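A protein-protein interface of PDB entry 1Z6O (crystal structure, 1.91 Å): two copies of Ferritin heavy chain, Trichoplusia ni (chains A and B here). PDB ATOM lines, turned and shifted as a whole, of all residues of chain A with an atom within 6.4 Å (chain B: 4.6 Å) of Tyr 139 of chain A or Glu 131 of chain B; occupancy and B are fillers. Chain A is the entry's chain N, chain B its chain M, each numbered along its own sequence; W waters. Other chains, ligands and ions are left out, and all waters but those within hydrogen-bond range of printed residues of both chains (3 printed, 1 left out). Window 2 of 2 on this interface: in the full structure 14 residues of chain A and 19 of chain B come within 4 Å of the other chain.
The backbone carbonyl oxygen of Val 142 of chain B sits at hydrogen-bond distance from the side-chain hydroxyl of Thr 146 of chain B. OH of Tyr 77 of chain A sits at hydrogen-bond distance from ND1 of His 140 of chain A (2.7 Å).
NH1 of Arg 124 of chain B is in hydrogen-bond range of O of Asn 137 of chain A (2.7 Å).
Water W2 lies within hydrogen-bond range of the side-chain carboxylate (OE1) of Glu 131 of chain B (2.7 Å), the side-chain hydroxyl (OH) of Tyr 139 of chain A (2.8 Å) and the side-chain carboxylate (OD2) of Asp 132 of chain B (2.8 Å). Water W3 lies within hydrogen-bond range of the side-chain carboxylate of Glu 131 of chain B (2.7 Å), the side-chain amide nitrogen of Asn 137 of chain A (2.9 Å) and the side-chain carboxylate of Glu 131 of chain A (3.2 Å). Water W1 bridges the backbone NH (N) of Asn 137 of chain A (2.8 Å) and the guanidinium group (NH2) of Arg 124 of chain B (3.0 Å).
Among the printed residues, merely in contact across the chains: Tyr 139 of chain A with Lys 128 of chain B, Phe 136 of chain A with Arg 124 of chain B, Tyr 139 of chain A with Thr 146 of chain B, Tyr 139 of chain A with Arg 124 of chain B, Tyr 139 of chain A with Ile 127 of chain B, Asp 143 of chain A with Thr 146 of chain B, His 140 of chain A with Thr 146 of chain B, His 140 of chain A with Leu 150 of chain B, Tyr 139 of chain A with Glu 131 of chain B and Tyr 139 of chain A with Leu 150 of chain B.
Hydrophobic or aromatic side chains of chain B that line the printed part of chain A: Ile 127 and Leu 150. Along chain A the printed residues that touch a printed residue of chain B span positions 136 to 143. Among the printed residues, no Asp or Glu carboxylate lies within 4 Å of a Lys or Arg side-chain nitrogen of the other chain.
5 positions are printed for both chains. Of the 11 pairs that touch across the chains among the printed residues, none has its exchanged pair printed and touching as well.
Of chain A, only Tyr 139 comes within 4 Å of Glu 131 of chain B. Of the printed residues of chain B, Asp 143 of chain A touches Thr 146. Of the printed residues of chain A, Ile 127 of chain B touches Tyr 139. Cys 130 of chain B touches none of the printed residues of chain A. Leu 141 of chain A touches none of the printed residues of chain B. The nearest residue of chain A that does not touch Glu 131 of chain B is Asn 137 of chain A (4.2 Å). The nearest printed residue of chain A that does not touch Leu 150 of chain B is Asp 138 of chain A (6.4 Å).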
ATOM      1  N   TYR A  77      15.816 -42.758  28.021  1.00  0.00           N
ATOM      2  CA  TYR A  77      16.946 -41.868  27.755  1.00  0.00           C
ATOM      3  C   TYR A  77      18.256 -42.625  28.046  1.00  0.00           C
ATOM      4  O   TYR A  77      19.192 -42.602  27.248  1.00  0.00           O
ATOM      5  CB  TYR A  77      16.870 -40.603  28.635  1.00  0.00           C
ATOM      6  CG  TYR A  77      17.935 -39.601  28.249  1.00  0.00           C
ATOM      7  CD1 TYR A  77      17.667 -38.605  27.308  1.00  0.00           C
ATOM      8  CD2 TYR A  77      19.248 -39.736  28.716  1.00  0.00           C
ATOM      9  CE1 TYR A  77      18.686 -37.771  26.826  1.00  0.00           C
ATOM     10  CE2 TYR A  77      20.276 -38.911  28.240  1.00  0.00           C
ATOM     11  CZ  TYR A  77      19.984 -37.938  27.291  1.00  0.00           C
ATOM     12  OH  TYR A  77      20.997 -37.171  26.755  1.00  0.00           O
ATOM     13  N   CYS A 130      24.646 -33.469  36.401  1.00  0.00           N
ATOM     14  CA  CYS A 130      24.977 -33.750  35.014  1.00  0.00           C
ATOM     15  C   CYS A 130      25.711 -32.617  34.320  1.00  0.00           C
ATOM     16  O   CYS A 130      26.509 -32.850  33.415  1.00  0.00           O
ATOM     17  CB  CYS A 130      23.696 -34.106  34.235  1.00  0.00           C
ATOM     18  SG  CYS A 130      22.943 -35.659  34.843  1.00  0.00           S
ATOM     19  N   GLU A 131      25.442 -31.390  34.741  1.00  0.00           N
ATOM     20  CA  GLU A 131      26.086 -30.242  34.124  1.00  0.00           C
ATOM     21  C   GLU A 131      27.434 -29.904  34.750  1.00  0.00           C
ATOM     22  O   GLU A 131      28.374 -29.553  34.048  1.00  0.00           O
ATOM     23  CB  GLU A 131      25.193 -28.995  34.243  1.00  0.00           C
ATOM     24  CG  GLU A 131      25.836 -27.731  33.669  1.00  0.00           C
ATOM     25  CD  GLU A 131      24.833 -26.599  33.456  1.00  0.00           C
ATOM     26  OE1 GLU A 131      24.633 -25.791  34.390  1.00  0.00           O
ATOM     27  OE2 GLU A 131      24.237 -26.526  32.353  1.00  0.00           O
ATOM     28  N   PHE A 136      32.854 -34.000  32.585  1.00  0.00           N
ATOM     29  CA  PHE A 136      31.943 -34.101  31.442  1.00  0.00           C
ATOM     30  C   PHE A 136      30.634 -33.364  31.711  1.00  0.00           C
ATOM     31  O   PHE A 136      29.877 -33.748  32.598  1.00  0.00           O
ATOM     32  CB  PHE A 136      31.644 -35.590  31.191  1.00  0.00           C
ATOM     33  CG  PHE A 136      30.899 -35.874  29.905  1.00  0.00           C
ATOM     34  CD1 PHE A 136      31.589 -36.021  28.702  1.00  0.00           C
ATOM     35  CD2 PHE A 136      29.511 -36.026  29.910  1.00  0.00           C
ATOM     36  CE1 PHE A 136      30.905 -36.321  27.507  1.00  0.00           C
ATOM     37  CE2 PHE A 136      28.812 -36.326  28.726  1.00  0.00           C
ATOM     38  CZ  PHE A 136      29.511 -36.473  27.521  1.00  0.00           C
ATOM     39  N   ASN A 137      30.391 -32.300  30.958  1.00  0.00           N
ATOM     40  CA  ASN A 137      29.156 -31.526  31.080  1.00  0.00           C
ATOM     41  C   ASN A 137      28.206 -32.216  30.086  1.00  0.00           C
ATOM     42  O   ASN A 137      28.429 -32.160  28.875  1.00  0.00           O
ATOM     43  CB  ASN A 137      29.414 -30.077  30.640  1.00  0.00           C
ATOM     44  CG  ASN A 137      28.173 -29.198  30.745  1.00  0.00           C
ATOM     45  OD1 ASN A 137      27.037 -29.683  30.646  1.00  0.00           O
ATOM     46  ND2 ASN A 137      28.384 -27.896  30.923  1.00  0.00           N
ATOM     47  N   ASP A 138      27.167 -32.878  30.578  1.00  0.00           N
ATOM     48  CA  ASP A 138      26.266 -33.580  29.659  1.00  0.00           C
ATOM     49  C   ASP A 138      25.221 -32.619  29.097  1.00  0.00           C
ATOM     50  O   ASP A 138      24.064 -32.606  29.530  1.00  0.00           O
ATOM     51  CB  ASP A 138      25.585 -34.740  30.379  1.00  0.00           C
ATOM     52  CG  ASP A 138      25.191 -35.846  29.421  1.00  0.00           C
ATOM     53  OD1 ASP A 138      24.586 -35.529  28.365  1.00  0.00           O
ATOM     54  OD2 ASP A 138      25.497 -37.021  29.713  1.00  0.00           O
ATOM     55  N   TYR A 139      25.630 -31.826  28.107  1.00  0.00           N
ATOM     56  CA  TYR A 139      24.746 -30.814  27.532  1.00  0.00           C
ATOM     57  C   TYR A 139      23.368 -31.313  27.119  1.00  0.00           C
ATOM     58  O   TYR A 139      22.352 -30.689  27.428  1.00  0.00           O
ATOM     59  CB  TYR A 139      25.400 -30.171  26.302  1.00  0.00           C
ATOM     60  CG  TYR A 139      26.738 -29.524  26.588  1.00  0.00           C
ATOM     61  CD1 TYR A 139      27.918 -30.068  26.079  1.00  0.00           C
ATOM     62  CD2 TYR A 139      26.820 -28.362  27.356  1.00  0.00           C
ATOM     63  CE1 TYR A 139      29.155 -29.468  26.324  1.00  0.00           C
ATOM     64  CE2 TYR A 139      28.058 -27.749  27.610  1.00  0.00           C
ATOM     65  CZ  TYR A 139      29.214 -28.312  27.086  1.00  0.00           C
ATOM     66  OH  TYR A 139      30.429 -27.705  27.301  1.00  0.00           O
ATOM     67  N   HIS A 140      23.340 -32.425  26.399  1.00  0.00           N
ATOM     68  CA  HIS A 140      22.075 -32.928  25.899  1.00  0.00           C
ATOM     69  C   HIS A 140      21.100 -33.383  26.973  1.00  0.00           C
ATOM     70  O   HIS A 140      19.913 -33.052  26.910  1.00  0.00           O
ATOM     71  CB  HIS A 140      22.309 -34.050  24.889  1.00  0.00           C
ATOM     72  CG  HIS A 140      21.049 -34.513  24.226  1.00  0.00           C
ATOM     73  ND1 HIS A 140      20.365 -35.639  24.634  1.00  0.00           N
ATOM     74  CD2 HIS A 140      20.316 -33.967  23.224  1.00  0.00           C
ATOM     75  CE1 HIS A 140      19.263 -35.770  23.910  1.00  0.00           C
ATOM     76  NE2 HIS A 140      19.208 -34.768  23.048  1.00  0.00           N
ATOM     77  N   LEU A 141      21.576 -34.132  27.962  1.00  0.00           N
ATOM     78  CA  LEU A 141      20.667 -34.579  29.016  1.00  0.00           C
ATOM     79  C   LEU A 141      20.185 -33.389  29.841  1.00  0.00           C
ATOM     80  O   LEU A 141      19.016 -33.318  30.211  1.00  0.00           O
ATOM     81  CB  LEU A 141      21.341 -35.626  29.923  1.00  0.00           C
ATOM     82  CG  LEU A 141      20.510 -36.103  31.139  1.00  0.00           C
ATOM     83  CD1 LEU A 141      19.106 -36.554  30.707  1.00  0.00           C
ATOM     84  CD2 LEU A 141      21.256 -37.261  31.827  1.00  0.00           C
ATOM     85  N   VAL A 142      21.078 -32.449  30.135  1.00  0.00           N
ATOM     86  CA  VAL A 142      20.681 -31.264  30.898  1.00  0.00           C
ATOM     87  C   VAL A 142      19.545 -30.537  30.159  1.00  0.00           C
ATOM     88  O   VAL A 142      18.542 -30.127  30.754  1.00  0.00           O
ATOM     89  CB  VAL A 142      21.896 -30.326  31.093  1.00  0.00           C
ATOM     90  CG1 VAL A 142      21.439 -28.927  31.566  1.00  0.00           C
ATOM     91  CG2 VAL A 142      22.856 -30.960  32.127  1.00  0.00           C
ATOM     92  N   ASP A 143      19.710 -30.403  28.850  1.00  0.00           N
ATOM     93  CA  ASP A 143      18.717 -29.743  28.000  1.00  0.00           C
ATOM     94  C   ASP A 143      17.391 -30.507  28.004  1.00  0.00           C
ATOM     95  O   ASP A 143      16.315 -29.910  28.066  1.00  0.00           O
ATOM     96  CB  ASP A 143      19.245 -29.668  26.565  1.00  0.00           C
ATOM     97  CG  ASP A 143      18.217 -29.094  25.602  1.00  0.00           C
ATOM     98  OD1 ASP A 143      18.053 -27.877  25.629  1.00  0.00           O
ATOM     99  OD2 ASP A 143      17.569 -29.859  24.853  1.00  0.00           O
ATOM    100  N   TYR A 144      17.468 -31.829  27.930  1.00  0.00           N
ATOM    101  CA  TYR A 144      16.275 -32.672  27.941  1.00  0.00           C
ATOM    102  C   TYR A 144      15.511 -32.533  29.266  1.00  0.00           C
ATOM    103  O   TYR A 144      14.283 -32.372  29.286  1.00  0.00           O
ATOM    104  CB  TYR A 144      16.685 -34.130  27.733  1.00  0.00           C
ATOM    105  CG  TYR A 144      15.526 -35.098  27.719  1.00  0.00           C
ATOM    106  CD1 TYR A 144      14.501 -34.973  26.776  1.00  0.00           C
ATOM    107  CD2 TYR A 144      15.463 -36.152  28.625  1.00  0.00           C
ATOM    108  CE1 TYR A 144      13.444 -35.883  26.733  1.00  0.00           C
ATOM    109  CE2 TYR A 144      14.407 -37.074  28.589  1.00  0.00           C
ATOM    110  CZ  TYR A 144      13.407 -36.929  27.638  1.00  0.00           C
ATOM    111  OH  TYR A 144      12.375 -37.837  27.582  1.00  0.00           O
ATOM    112  N   ARG B 124      30.227 -31.051  20.723  1.00  0.00           N
ATOM    113  CA  ARG B 124      30.363 -30.696  22.137  1.00  0.00           C
ATOM    114  C   ARG B 124      31.531 -29.708  22.297  1.00  0.00           C
ATOM    115  O   ARG B 124      31.483 -28.817  23.148  1.00  0.00           O
ATOM    116  CB  ARG B 124      30.567 -31.962  23.001  1.00  0.00           C
ATOM    117  CG  ARG B 124      29.269 -32.821  23.161  1.00  0.00           C
ATOM    118  CD  ARG B 124      29.569 -34.158  23.874  1.00  0.00           C
ATOM    119  NE  ARG B 124      30.384 -33.883  25.048  1.00  0.00           N
ATOM    120  CZ  ARG B 124      29.909 -33.462  26.213  1.00  0.00           C
ATOM    121  NH1 ARG B 124      28.602 -33.305  26.395  1.00  0.00           N
ATOM    122  NH2 ARG B 124      30.753 -33.081  27.161  1.00  0.00           N
ATOM    123  N   ILE B 127      30.312 -26.322  21.257  1.00  0.00           N
ATOM    124  CA  ILE B 127      29.504 -25.802  22.355  1.00  0.00           C
ATOM    125  C   ILE B 127      30.420 -25.202  23.440  1.00  0.00           C
ATOM    126  O   ILE B 127      30.180 -24.089  23.928  1.00  0.00           O
ATOM    127  CB  ILE B 127      28.618 -26.930  22.959  1.00  0.00           C
ATOM    128  CG1 ILE B 127      27.449 -27.220  21.999  1.00  0.00           C
ATOM    129  CG2 ILE B 127      28.097 -26.525  24.342  1.00  0.00           C
ATOM    130  CD1 ILE B 127      26.688 -28.516  22.335  1.00  0.00           C
ATOM    131  N   LYS B 128      31.471 -25.929  23.809  1.00  0.00           N
ATOM    132  CA  LYS B 128      32.407 -25.424  24.823  1.00  0.00           C
ATOM    133  C   LYS B 128      33.039 -24.103  24.392  1.00  0.00           C
ATOM    134  O   LYS B 128      33.115 -23.157  25.179  1.00  0.00           O
ATOM    135  CB  LYS B 128      33.542 -26.422  25.090  1.00  0.00           C
ATOM    136  CG  LYS B 128      33.124 -27.738  25.674  1.00  0.00           C
ATOM    137  CD  LYS B 128      34.354 -28.553  26.075  1.00  0.00           C
ATOM    138  CE  LYS B 128      33.985 -29.994  26.420  1.00  0.00           C
ATOM    139  NZ  LYS B 128      33.577 -30.780  25.217  1.00  0.00           N
ATOM    140  N   ALA B 129      33.512 -24.042  23.152  1.00  0.00           N
ATOM    141  CA  ALA B 129      34.129 -22.814  22.656  1.00  0.00           C
ATOM    142  C   ALA B 129      33.149 -21.641  22.666  1.00  0.00           C
ATOM    143  O   ALA B 129      33.508 -20.519  23.030  1.00  0.00           O
ATOM    144  CB  ALA B 129      34.666 -23.024  21.229  1.00  0.00           C
ATOM    145  N   CYS B 130      31.906 -21.902  22.268  1.00  0.00           N
ATOM    146  CA  CYS B 130      30.898 -20.856  22.191  1.00  0.00           C
ATOM    147  C   CYS B 130      30.356 -20.429  23.543  1.00  0.00           C
ATOM    148  O   CYS B 130      29.962 -19.280  23.724  1.00  0.00           O
ATOM    149  CB  CYS B 130      29.743 -21.314  21.280  1.00  0.00           C
ATOM    150  SG  CYS B 130      30.294 -21.539  19.550  1.00  0.00           S
ATOM    151  N   GLU B 131      30.336 -21.352  24.492  1.00  0.00           N
ATOM    152  CA  GLU B 131      29.820 -21.037  25.816  1.00  0.00           C
ATOM    153  C   GLU B 131      30.875 -20.447  26.744  1.00  0.00           C
ATOM    154  O   GLU B 131      30.589 -19.530  27.504  1.00  0.00           O
ATOM    155  CB  GLU B 131      29.262 -22.302  26.490  1.00  0.00           C
ATOM    156  CG  GLU B 131      28.757 -22.057  27.914  1.00  0.00           C
ATOM    157  CD  GLU B 131      27.888 -23.197  28.439  1.00  0.00           C
ATOM    158  OE1 GLU B 131      28.438 -24.141  29.047  1.00  0.00           O
ATOM    159  OE2 GLU B 131      26.649 -23.151  28.233  1.00  0.00           O
ATOM    160  N   ASP B 132      32.094 -20.965  26.668  1.00  0.00           N
ATOM    161  CA  ASP B 132      33.130 -20.535  27.594  1.00  0.00           C
ATOM    162  C   ASP B 132      34.059 -19.401  27.214  1.00  0.00           C
ATOM    163  O   ASP B 132      35.004 -19.122  27.938  1.00  0.00           O
ATOM    164  CB  ASP B 132      33.949 -21.748  28.033  1.00  0.00           C
ATOM    165  CG  ASP B 132      33.093 -22.785  28.762  1.00  0.00           C
ATOM    166  OD1 ASP B 132      32.212 -22.383  29.556  1.00  0.00           O
ATOM    167  OD2 ASP B 132      33.305 -23.992  28.550  1.00  0.00           O
ATOM    168  N   ASP B 133      33.802 -18.745  26.089  1.00  0.00           N
ATOM    169  CA  ASP B 133      34.625 -17.607  25.693  1.00  0.00           C
ATOM    170  C   ASP B 133      34.421 -16.573  26.816  1.00  0.00           C
ATOM    171  O   ASP B 133      33.296 -16.158  27.085  1.00  0.00           O
ATOM    172  CB  ASP B 133      34.127 -17.042  24.365  1.00  0.00           C
ATOM    173  CG  ASP B 133      35.003 -15.917  23.850  1.00  0.00           C
ATOM    174  OD1 ASP B 133      35.272 -14.973  24.624  1.00  0.00           O
ATOM    175  OD2 ASP B 133      35.419 -15.980  22.675  1.00  0.00           O
ATOM    176  N   ASN B 137      29.367 -15.335  26.068  1.00  0.00           N
ATOM    177  CA  ASN B 137      28.769 -16.666  26.165  1.00  0.00           C
ATOM    178  C   ASN B 137      27.644 -16.624  25.118  1.00  0.00           C
ATOM    179  O   ASN B 137      26.669 -15.889  25.285  1.00  0.00           O
ATOM    180  CB  ASN B 137      28.175 -16.859  27.568  1.00  0.00           C
ATOM    181  CG  ASN B 137      27.536 -18.230  27.755  1.00  0.00           C
ATOM    182  OD1 ASN B 137      27.066 -18.853  26.791  1.00  0.00           O
ATOM    183  ND2 ASN B 137      27.493 -18.698  29.000  1.00  0.00           N
ATOM    184  N   ASP B 138      27.772 -17.384  24.038  1.00  0.00           N
ATOM    185  CA  ASP B 138      26.735 -17.338  23.003  1.00  0.00           C
ATOM    186  C   ASP B 138      25.579 -18.269  23.362  1.00  0.00           C
ATOM    187  O   ASP B 138      25.456 -19.374  22.821  1.00  0.00           O
ATOM    188  CB  ASP B 138      27.327 -17.726  21.652  1.00  0.00           C
ATOM    189  CG  ASP B 138      26.565 -17.102  20.500  1.00  0.00           C
ATOM    190  OD1 ASP B 138      25.311 -17.187  20.504  1.00  0.00           O
ATOM    191  OD2 ASP B 138      27.214 -16.519  19.607  1.00  0.00           O
ATOM    192  N   VAL B 142      24.660 -22.027  21.542  1.00  0.00           N
ATOM    193  CA  VAL B 142      24.893 -23.197  22.391  1.00  0.00           C
ATOM    194  C   VAL B 142      23.595 -24.014  22.502  1.00  0.00           C
ATOM    195  O   VAL B 142      23.591 -25.244  22.384  1.00  0.00           O
ATOM    196  CB  VAL B 142      25.380 -22.750  23.790  1.00  0.00           C
ATOM    197  CG1 VAL B 142      25.286 -23.915  24.803  1.00  0.00           C
ATOM    198  CG2 VAL B 142      26.840 -22.249  23.676  1.00  0.00           C
ATOM    199  N   THR B 146      22.861 -27.760  21.067  1.00  0.00           N
ATOM    200  CA  THR B 146      22.497 -28.772  22.047  1.00  0.00           C
ATOM    201  C   THR B 146      21.138 -29.418  21.755  1.00  0.00           C
ATOM    202  O   THR B 146      21.017 -30.644  21.729  1.00  0.00           O
ATOM    203  CB  THR B 146      22.454 -28.178  23.473  1.00  0.00           C
ATOM    204  OG1 THR B 146      23.735 -27.626  23.805  1.00  0.00           O
ATOM    205  CG2 THR B 146      22.106 -29.263  24.493  1.00  0.00           C
ATOM    206  N   LEU B 150      22.845 -32.072  18.845  1.00  0.00           N
ATOM    207  CA  LEU B 150      23.141 -33.213  19.719  1.00  0.00           C
ATOM    208  C   LEU B 150      21.965 -34.186  19.771  1.00  0.00           C
ATOM    209  O   LEU B 150      22.158 -35.396  19.864  1.00  0.00           O
ATOM    210  CB  LEU B 150      23.513 -32.752  21.136  1.00  0.00           C
ATOM    211  CG  LEU B 150      24.901 -32.100  21.258  1.00  0.00           C
ATOM    212  CD1 LEU B 150      25.220 -31.837  22.748  1.00  0.00           C
ATOM    213  CD2 LEU B 150      25.969 -33.035  20.657  1.00  0.00           C
HETATM  214  O   HOH W   1      32.431 -31.516  29.130  1.00  0.00           O
HETATM  215  O   HOH W   2      30.797 -25.306  28.613  1.00  0.00           O
HETATM  216  O   HOH W   3      26.685 -25.581  30.600  1.00  0.00           O
